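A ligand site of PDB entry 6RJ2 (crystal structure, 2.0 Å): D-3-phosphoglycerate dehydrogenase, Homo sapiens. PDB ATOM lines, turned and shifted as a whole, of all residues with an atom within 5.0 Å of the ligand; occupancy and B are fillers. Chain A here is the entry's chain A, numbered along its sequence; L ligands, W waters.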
ATOM      1  N   PRO A  98      -2.785  31.091  -4.242  1.00  0.00           N
ATOM      2  CA  PRO A  98      -1.352  31.263  -4.551  1.00  0.00           C
ATOM      3  C   PRO A  98      -0.996  31.226  -6.041  1.00  0.00           C
ATOM      4  O   PRO A  98       0.009  31.820  -6.434  1.00  0.00           O
ATOM      5  CB  PRO A  98      -0.678  30.137  -3.763  1.00  0.00           C
ATOM      6  CG  PRO A  98      -1.732  29.101  -3.593  1.00  0.00           C
ATOM      7  CD  PRO A  98      -3.024  29.848  -3.484  1.00  0.00           C
ATOM      8  N   ASN A  99      -1.822  30.549  -6.868  1.00  0.00           N
ATOM      9  CA  ASN A  99      -1.605  30.453  -8.307  1.00  0.00           C
ATOM     10  C   ASN A  99      -1.804  31.778  -9.047  1.00  0.00           C
ATOM     11  O   ASN A  99      -1.121  32.026 -10.037  1.00  0.00           O
ATOM     12  CB  ASN A  99      -2.473  29.342  -8.922  1.00  0.00           C
ATOM     13  CG  ASN A  99      -2.071  27.931  -8.525  1.00  0.00           C
ATOM     14  OD1 ASN A  99      -1.189  27.688  -7.680  1.00  0.00           O
ATOM     15  ND2 ASN A  99      -2.727  26.942  -9.134  1.00  0.00           N
ATOM     16  N   SER A 102       1.414  33.621  -9.072  1.00  0.00           N
ATOM     17  CA  SER A 102       2.523  32.874  -9.669  1.00  0.00           C
ATOM     18  C   SER A 102       3.385  33.674 -10.618  1.00  0.00           C
ATOM     19  O   SER A 102       4.600  33.723 -10.411  1.00  0.00           O
ATOM     20  CB  SER A 102       2.015  31.606 -10.343  1.00  0.00           C
ATOM     21  OG  SER A 102       1.686  30.663  -9.336  1.00  0.00           O
ATOM     22  N   LEU A 150      14.941  25.497  -5.869  1.00  0.00           N
ATOM     23  CA  LEU A 150      14.436  24.639  -4.801  1.00  0.00           C
ATOM     24  C   LEU A 150      12.963  24.947  -4.604  1.00  0.00           C
ATOM     25  O   LEU A 150      12.607  26.028  -4.139  1.00  0.00           O
ATOM     26  CB  LEU A 150      15.266  24.846  -3.517  1.00  0.00           C
ATOM     27  CG  LEU A 150      16.798  24.841  -3.689  1.00  0.00           C
ATOM     28  CD1 LEU A 150      17.470  25.126  -2.371  1.00  0.00           C
ATOM     29  CD2 LEU A 150      17.309  23.517  -4.270  1.00  0.00           C
ATOM     30  N   GLY A 151      12.140  24.000  -5.029  1.00  0.00           N
ATOM     31  CA  GLY A 151      10.690  24.103  -5.049  1.00  0.00           C
ATOM     32  C   GLY A 151      10.282  24.247  -6.494  1.00  0.00           C
ATOM     33  O   GLY A 151      10.686  25.196  -7.156  1.00  0.00           O
ATOM     34  N   LEU A 152       9.562  23.251  -7.023  1.00  0.00           N
ATOM     35  CA  LEU A 152       9.215  23.257  -8.439  1.00  0.00           C
ATOM     36  C   LEU A 152       7.717  23.260  -8.699  1.00  0.00           C
ATOM     37  O   LEU A 152       7.231  22.563  -9.586  1.00  0.00           O
ATOM     38  CB  LEU A 152       9.938  22.125  -9.202  1.00  0.00           C
ATOM     39  CG  LEU A 152      11.487  22.149  -9.141  1.00  0.00           C
ATOM     40  CD1 LEU A 152      12.067  20.842  -9.576  1.00  0.00           C
ATOM     41  CD2 LEU A 152      12.064  23.266 -10.012  1.00  0.00           C
ATOM     42  N   GLY A 153       7.003  24.115  -7.967  1.00  0.00           N
ATOM     43  CA  GLY A 153       5.584  24.391  -8.194  1.00  0.00           C
ATOM     44  C   GLY A 153       5.484  25.308  -9.405  1.00  0.00           C
ATOM     45  O   GLY A 153       6.439  25.415 -10.177  1.00  0.00           O
ATOM     46  N   ARG A 154       4.342  26.006  -9.587  1.00  0.00           N
ATOM     47  CA  ARG A 154       4.155  26.926 -10.720  1.00  0.00           C
ATOM     48  C   ARG A 154       5.182  28.086 -10.729  1.00  0.00           C
ATOM     49  O   ARG A 154       5.717  28.408 -11.788  1.00  0.00           O
ATOM     50  CB  ARG A 154       2.682  27.420 -10.808  1.00  0.00           C
ATOM     51  CG  ARG A 154       2.311  28.293 -12.033  1.00  0.00           C
ATOM     52  CD  ARG A 154       2.753  27.787 -13.401  1.00  0.00           C
ATOM     53  NE  ARG A 154       2.192  26.476 -13.747  1.00  0.00           N
ATOM     54  CZ  ARG A 154       2.365  25.877 -14.930  1.00  0.00           C
ATOM     55  NH1 ARG A 154       1.838  24.688 -15.155  1.00  0.00           N
ATOM     56  NH2 ARG A 154       3.080  26.462 -15.881  1.00  0.00           N
ATOM     57  N   ILE A 155       5.526  28.655  -9.569  1.00  0.00           N
ATOM     58  CA  ILE A 155       6.525  29.734  -9.531  1.00  0.00           C
ATOM     59  C   ILE A 155       7.908  29.228  -9.992  1.00  0.00           C
ATOM     60  O   ILE A 155       8.486  29.798 -10.916  1.00  0.00           O
ATOM     61  CB  ILE A 155       6.569  30.496  -8.175  1.00  0.00           C
ATOM     62  CG1 ILE A 155       5.154  31.039  -7.811  1.00  0.00           C
ATOM     63  CG2 ILE A 155       7.583  31.646  -8.260  1.00  0.00           C
ATOM     64  CD1 ILE A 155       4.962  31.467  -6.322  1.00  0.00           C
ATOM     65  N   GLY A 156       8.363  28.114  -9.413  1.00  0.00           N
ATOM     66  CA  GLY A 156       9.634  27.453  -9.735  1.00  0.00           C
ATOM     67  C   GLY A 156       9.803  27.171 -11.213  1.00  0.00           C
ATOM     68  O   GLY A 156      10.842  27.509 -11.793  1.00  0.00           O
ATOM     69  N   TYR A 173      15.257  20.819  -7.230  1.00  0.00           N
ATOM     70  CA  TYR A 173      14.758  19.732  -6.393  1.00  0.00           C
ATOM     71  C   TYR A 173      13.407  20.104  -5.832  1.00  0.00           C
ATOM     72  O   TYR A 173      13.171  21.236  -5.426  1.00  0.00           O
ATOM     73  CB  TYR A 173      15.738  19.402  -5.245  1.00  0.00           C
ATOM     74  CG  TYR A 173      15.262  18.328  -4.296  1.00  0.00           C
ATOM     75  CD1 TYR A 173      15.421  16.974  -4.604  1.00  0.00           C
ATOM     76  CD2 TYR A 173      14.647  18.653  -3.096  1.00  0.00           C
ATOM     77  CE1 TYR A 173      14.983  15.976  -3.723  1.00  0.00           C
ATOM     78  CE2 TYR A 173      14.191  17.669  -2.212  1.00  0.00           C
ATOM     79  CZ  TYR A 173      14.357  16.336  -2.543  1.00  0.00           C
ATOM     80  OH  TYR A 173      13.909  15.365  -1.675  1.00  0.00           O
ATOM     81  N   ASP A 174      12.546  19.114  -5.800  1.00  0.00           N
ATOM     82  CA  ASP A 174      11.218  19.171  -5.221  1.00  0.00           C
ATOM     83  C   ASP A 174      10.798  17.723  -4.956  1.00  0.00           C
ATOM     84  O   ASP A 174      10.741  16.932  -5.907  1.00  0.00           O
ATOM     85  CB  ASP A 174      10.211  19.905  -6.122  1.00  0.00           C
ATOM     86  CG  ASP A 174       8.896  20.177  -5.415  1.00  0.00           C
ATOM     87  OD1 ASP A 174       8.209  19.199  -5.041  1.00  0.00           O
ATOM     88  OD2 ASP A 174       8.553  21.362  -5.242  1.00  0.00           O
ATOM     89  N   PRO A 175      10.539  17.343  -3.688  1.00  0.00           N
ATOM     90  CA  PRO A 175      10.153  15.942  -3.398  1.00  0.00           C
ATOM     91  C   PRO A 175       8.753  15.557  -3.857  1.00  0.00           C
ATOM     92  O   PRO A 175       8.421  14.380  -3.808  1.00  0.00           O
ATOM     93  CB  PRO A 175      10.308  15.852  -1.876  1.00  0.00           C
ATOM     94  CG  PRO A 175      10.001  17.217  -1.392  1.00  0.00           C
ATOM     95  CD  PRO A 175      10.567  18.150  -2.450  1.00  0.00           C
ATOM     96  N   ILE A 176       7.916  16.532  -4.285  1.00  0.00           N
ATOM     97  CA  ILE A 176       6.561  16.260  -4.784  1.00  0.00           C
ATOM     98  C   ILE A 176       6.585  16.111  -6.303  1.00  0.00           C
ATOM     99  O   ILE A 176       5.874  15.257  -6.847  1.00  0.00           O
ATOM    100  CB  ILE A 176       5.511  17.319  -4.312  1.00  0.00           C
ATOM    101  CG1 ILE A 176       5.465  17.423  -2.782  1.00  0.00           C
ATOM    102  CG2 ILE A 176       4.111  17.035  -4.920  1.00  0.00           C
ATOM    103  CD1 ILE A 176       4.448  18.445  -2.230  1.00  0.00           C
ATOM    104  N   ILE A 177       7.379  16.951  -6.981  1.00  0.00           N
ATOM    105  CA  ILE A 177       7.494  16.971  -8.439  1.00  0.00           C
ATOM    106  C   ILE A 177       8.456  15.871  -8.907  1.00  0.00           C
ATOM    107  O   ILE A 177       9.592  15.797  -8.425  1.00  0.00           O
ATOM    108  CB  ILE A 177       7.877  18.399  -8.956  1.00  0.00           C
ATOM    109  CG1 ILE A 177       6.859  19.491  -8.494  1.00  0.00           C
ATOM    110  CG2 ILE A 177       8.112  18.425 -10.483  1.00  0.00           C
ATOM    111  CD1 ILE A 177       5.316  19.299  -8.887  1.00  0.00           C
ATOM    112  N   LEU A 192      19.288  17.238  -3.098  1.00  0.00           N
ATOM    113  CA  LEU A 192      19.723  18.505  -2.485  1.00  0.00           C
ATOM    114  C   LEU A 192      21.236  18.657  -2.321  1.00  0.00           C
ATOM    115  O   LEU A 192      21.771  19.696  -2.700  1.00  0.00           O
ATOM    116  CB  LEU A 192      19.042  18.733  -1.126  1.00  0.00           C
ATOM    117  CG  LEU A 192      17.735  19.533  -1.096  1.00  0.00           C
ATOM    118  CD1 LEU A 192      17.221  19.618   0.324  1.00  0.00           C
ATOM    119  CD2 LEU A 192      17.921  20.963  -1.656  1.00  0.00           C
ATOM    120  N   HIS A 205      11.468  28.516  -3.907  1.00  0.00           N
ATOM    121  CA  HIS A 205      10.051  28.647  -4.239  1.00  0.00           C
ATOM    122  C   HIS A 205       9.327  27.469  -3.613  1.00  0.00           C
ATOM    123  O   HIS A 205       8.795  26.621  -4.313  1.00  0.00           O
ATOM    124  CB  HIS A 205       9.850  28.672  -5.775  1.00  0.00           C
ATOM    125  CG  HIS A 205      10.676  29.719  -6.433  1.00  0.00           C
ATOM    126  ND1 HIS A 205      10.365  31.051  -6.302  1.00  0.00           N
ATOM    127  CD2 HIS A 205      11.859  29.613  -7.077  1.00  0.00           C
ATOM    128  CE1 HIS A 205      11.317  31.714  -6.930  1.00  0.00           C
ATOM    129  NE2 HIS A 205      12.247  30.885  -7.403  1.00  0.00           N
ATOM    130  N   THR A 206       9.376  27.392  -2.276  1.00  0.00           N
ATOM    131  CA  THR A 206       8.750  26.303  -1.545  1.00  0.00           C
ATOM    132  C   THR A 206       7.738  26.878  -0.572  1.00  0.00           C
ATOM    133  O   THR A 206       7.841  28.052  -0.244  1.00  0.00           O
ATOM    134  CB  THR A 206       9.815  25.554  -0.701  1.00  0.00           C
ATOM    135  OG1 THR A 206      10.351  26.428   0.295  1.00  0.00           O
ATOM    136  CG2 THR A 206      10.906  24.930  -1.530  1.00  0.00           C
ATOM    137  N   PRO A 207       6.828  26.063   0.000  1.00  0.00           N
ATOM    138  CA  PRO A 207       6.019  26.587   1.116  1.00  0.00           C
ATOM    139  C   PRO A 207       6.948  26.703   2.338  1.00  0.00           C
ATOM    140  O   PRO A 207       8.072  26.174   2.298  1.00  0.00           O
ATOM    141  CB  PRO A 207       4.962  25.491   1.341  1.00  0.00           C
ATOM    142  CG  PRO A 207       5.582  24.245   0.849  1.00  0.00           C
ATOM    143  CD  PRO A 207       6.555  24.621  -0.232  1.00  0.00           C
ATOM    144  N   LEU A 209       7.657  25.303   5.813  1.00  0.00           N
ATOM    145  CA  LEU A 209       7.345  24.119   6.638  1.00  0.00           C
ATOM    146  C   LEU A 209       8.572  23.740   7.469  1.00  0.00           C
ATOM    147  O   LEU A 209       9.666  24.191   7.112  1.00  0.00           O
ATOM    148  CB  LEU A 209       6.994  22.936   5.699  1.00  0.00           C
ATOM    149  CG  LEU A 209       5.840  23.082   4.690  1.00  0.00           C
ATOM    150  CD1 LEU A 209       5.825  21.902   3.756  1.00  0.00           C
ATOM    151  CD2 LEU A 209       4.481  23.227   5.386  1.00  0.00           C
ATOM    152  N   SER A 211      10.418  21.214   7.268  1.00  0.00           N
ATOM    153  CA  SER A 211      11.334  20.669   6.262  1.00  0.00           C
ATOM    154  C   SER A 211      12.048  21.770   5.423  1.00  0.00           C
ATOM    155  O   SER A 211      13.122  21.509   4.882  1.00  0.00           O
ATOM    156  CB  SER A 211      10.596  19.715   5.329  1.00  0.00           C
ATOM    157  OG  SER A 211       9.570  20.402   4.631  1.00  0.00           O
ATOM    158  N   THR A 212      11.433  22.973   5.318  1.00  0.00           N
ATOM    159  CA  THR A 212      11.999  24.072   4.522  1.00  0.00           C
ATOM    160  C   THR A 212      12.535  25.236   5.369  1.00  0.00           C
ATOM    161  O   THR A 212      13.143  26.141   4.810  1.00  0.00           O
ATOM    162  CB  THR A 212      11.022  24.567   3.457  1.00  0.00           C
ATOM    163  OG1 THR A 212       9.847  25.058   4.090  1.00  0.00           O
ATOM    164  CG2 THR A 212      10.668  23.499   2.438  1.00  0.00           C
ATOM    165  N   LEU A 215      16.437  25.973   5.093  1.00  0.00           N
ATOM    166  CA  LEU A 215      16.866  25.090   4.008  1.00  0.00           C
ATOM    167  C   LEU A 215      18.266  25.535   3.548  1.00  0.00           C
ATOM    168  O   LEU A 215      19.133  24.699   3.284  1.00  0.00           O
ATOM    169  CB  LEU A 215      15.836  25.174   2.857  1.00  0.00           C
ATOM    170  CG  LEU A 215      15.946  24.151   1.722  1.00  0.00           C
ATOM    171  CD1 LEU A 215      15.687  22.728   2.216  1.00  0.00           C
ATOM    172  CD2 LEU A 215      14.983  24.497   0.593  1.00  0.00           C
ATOM    173  N   ARG A 235       9.165  32.818   1.023  1.00  0.00           N
ATOM    174  CA  ARG A 235       8.729  33.078   2.399  1.00  0.00           C
ATOM    175  C   ARG A 235       9.928  33.272   3.303  1.00  0.00           C
ATOM    176  O   ARG A 235      10.955  32.615   3.124  1.00  0.00           O
ATOM    177  CB  ARG A 235       7.843  31.934   2.938  1.00  0.00           C
ATOM    178  CG  ARG A 235       6.394  31.988   2.460  1.00  0.00           C
ATOM    179  CD  ARG A 235       5.795  30.605   2.385  1.00  0.00           C
ATOM    180  NE  ARG A 235       4.555  30.564   1.601  1.00  0.00           N
ATOM    181  CZ  ARG A 235       4.489  30.183   0.329  1.00  0.00           C
ATOM    182  NH1 ARG A 235       5.572  29.789  -0.317  1.00  0.00           N
ATOM    183  NH2 ARG A 235       3.322  30.179  -0.299  1.00  0.00           N
HETATM  184  C1  LIG L   1       3.739  23.909  -4.219  1.00  0.00           C
HETATM  185  C2  LIG L   1       5.150  21.349  -5.977  1.00  0.00           C
HETATM  186  C3  LIG L   1       6.111  25.365  -4.253  1.00  0.00           C
HETATM  187  C4  LIG L   1       3.714  25.287  -4.072  1.00  0.00           C
HETATM  188  C5  LIG L   1       6.143  21.342  -2.383  1.00  0.00           C
HETATM  189  C6  LIG L   1       9.492  21.074  -0.942  1.00  0.00           C
HETATM  190  C7  LIG L   1       6.385  20.095   0.484  1.00  0.00           C
HETATM  191  C8  LIG L   1      13.064  20.955   0.261  1.00  0.00           C
HETATM  192  C9  LIG L   1      13.750  21.408  -0.857  1.00  0.00           C
HETATM  193  C10 LIG L   1      13.049  21.749  -2.017  1.00  0.00           C
HETATM  194  C11 LIG L   1       3.608  28.177  -6.187  1.00  0.00           C
HETATM  195  C12 LIG L   1       4.959  23.259  -4.407  1.00  0.00           C
HETATM  196  C13 LIG L   1       5.007  21.750  -4.512  1.00  0.00           C
HETATM  197  C14 LIG L   1       6.136  23.987  -4.399  1.00  0.00           C
HETATM  198  N1  LIG L   1       6.197  21.363  -3.736  1.00  0.00           N
HETATM  199  C15 LIG L   1       4.906  26.016  -4.080  1.00  0.00           C
HETATM  200  O1  LIG L   1       5.097  21.577  -1.798  1.00  0.00           O
HETATM  201  C16 LIG L   1       7.381  21.072  -1.623  1.00  0.00           C
HETATM  202  N2  LIG L   1       7.487  20.563  -0.361  1.00  0.00           N
HETATM  203  N3  LIG L   1       8.727  20.548  -0.010  1.00  0.00           N
HETATM  204  C17 LIG L   1       8.656  21.445  -2.018  1.00  0.00           C
HETATM  205  C18 LIG L   1      10.970  21.203  -0.902  1.00  0.00           C
HETATM  206  C19 LIG L   1      11.676  20.836   0.242  1.00  0.00           C
HETATM  207  C20 LIG L   1      11.669  21.627  -2.042  1.00  0.00           C
HETATM  208  S1  LIG L   1       4.880  27.775  -3.917  1.00  0.00           S
HETATM  209  O2  LIG L   1       4.549  28.069  -2.572  1.00  0.00           O
HETATM  210  O3  LIG L   1       6.088  28.214  -4.547  1.00  0.00           O
HETATM  211  N4  LIG L   1       3.608  28.279  -4.844  1.00  0.00           N
HETATM  212  O4  LIG L   1       4.567  27.710  -6.785  1.00  0.00           O
HETATM  213  C21 LIG L   1       2.397  28.649  -6.950  1.00  0.00           C
HETATM  214  O   HOH W   1       2.786  23.826  -1.026  1.00  0.00           O
HETATM  215  O   HOH W   2       6.905  30.533  -3.184  1.00  0.00           O
HETATM  216  O   HOH W   3       9.610  19.159   2.235  1.00  0.00           O
HETATM  217  O   HOH W   4       7.239  26.910  -6.817  1.00  0.00           O
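An oxygen (O2) of the ligand sits at hydrogen-bond distance from the guanidinium group (NH1) of Arg 235, 3.0 Å away.
The backbone NH (N) of Ile 155 sits at hydrogen-bond distance from an oxygen (O4) of the ligand (3.1 Å).
N of Arg 154 sits at hydrogen-bond distance from O4 of the ligand (3.3 Å).
A nitrogen (N1) of the ligand is in hydrogen-bond range of the side-chain carboxylate of Asp 174, 2.8 Å away.
O of Leu 150 lies within hydrogen-bond range of N of His 205, 2.7 Å away.
OG of Ser 102 sits close to O of Asn 99 (3.2 Å).
The side-chain hydroxyl (OG1) of Thr 212 sits at hydrogen-bond distance from the backbone carbonyl oxygen (O) of Pro 207, at 2.8 Å.
O of Tyr 173 is in hydrogen-bond range of N of Gly 151 (3.0 Å).
OD2 of Asp 174 sits at hydrogen-bond distance from N of Leu 152, 2.8 Å away.
OD1 of Asp 174 is in hydrogen-bond range of N of Ile 176 (2.8 Å).
The backbone NH of Ile 177 lies within hydrogen-bond range of the side-chain carboxylate of Asp 174 (3.1 Å).
N of Leu 209 sits at hydrogen-bond distance from OG1 of Thr 212, 2.8 Å away.
O3 of the ligand lies close to O of His 205.
Merely in contact with the ligand: Asn 99 (3.8 Å), Ser 102 (3.2 Å), Gly 151 (3.8 Å), Gly 153 (3.7 Å), Tyr 173 (3.4 Å), Pro 175 (3.4 Å), Ile 176 (3.2 Å), Ile 177 (3.6 Å), Thr 206 (3.4 Å), Pro 207 (3.7 Å), Leu 209 (3.8 Å), Thr 212 (3.6 Å) and Leu 215 (3.6 Å).
Hydrophobic or aromatic side chains within 4 Å of the ligand: Ile 155, Tyr 173, Pro 175, Ile 176, Ile 177, His 205, Pro 207, Leu 209 and Leu 215.
Within 4 Å of the ligand: Asn 99, Ser 102, Gly 151, Gly 153, Arg 154, Ile 155, Tyr 173, Asp 174, Pro 175, Ile 176, Ile 177, His 205, Thr 206, Pro 207, Leu 209, Thr 212, Leu 215 and Arg 235.
Water W3 bridges the side-chain hydroxyl of Ser 211 (2.7 Å) and a nitrogen (N3) of the ligand (2.8 Å).
Water W4 lies within hydrogen-bond range of O4 of the ligand (2.8 Å), O of His 205 (3.0 Å), N of Gly 153 (3.0 Å) and N of Gly 156 (3.1 Å).
Water W2 bridges an oxygen (O3) of the ligand (2.8 Å) and the guanidinium group of Arg 235 (3.2 Å).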
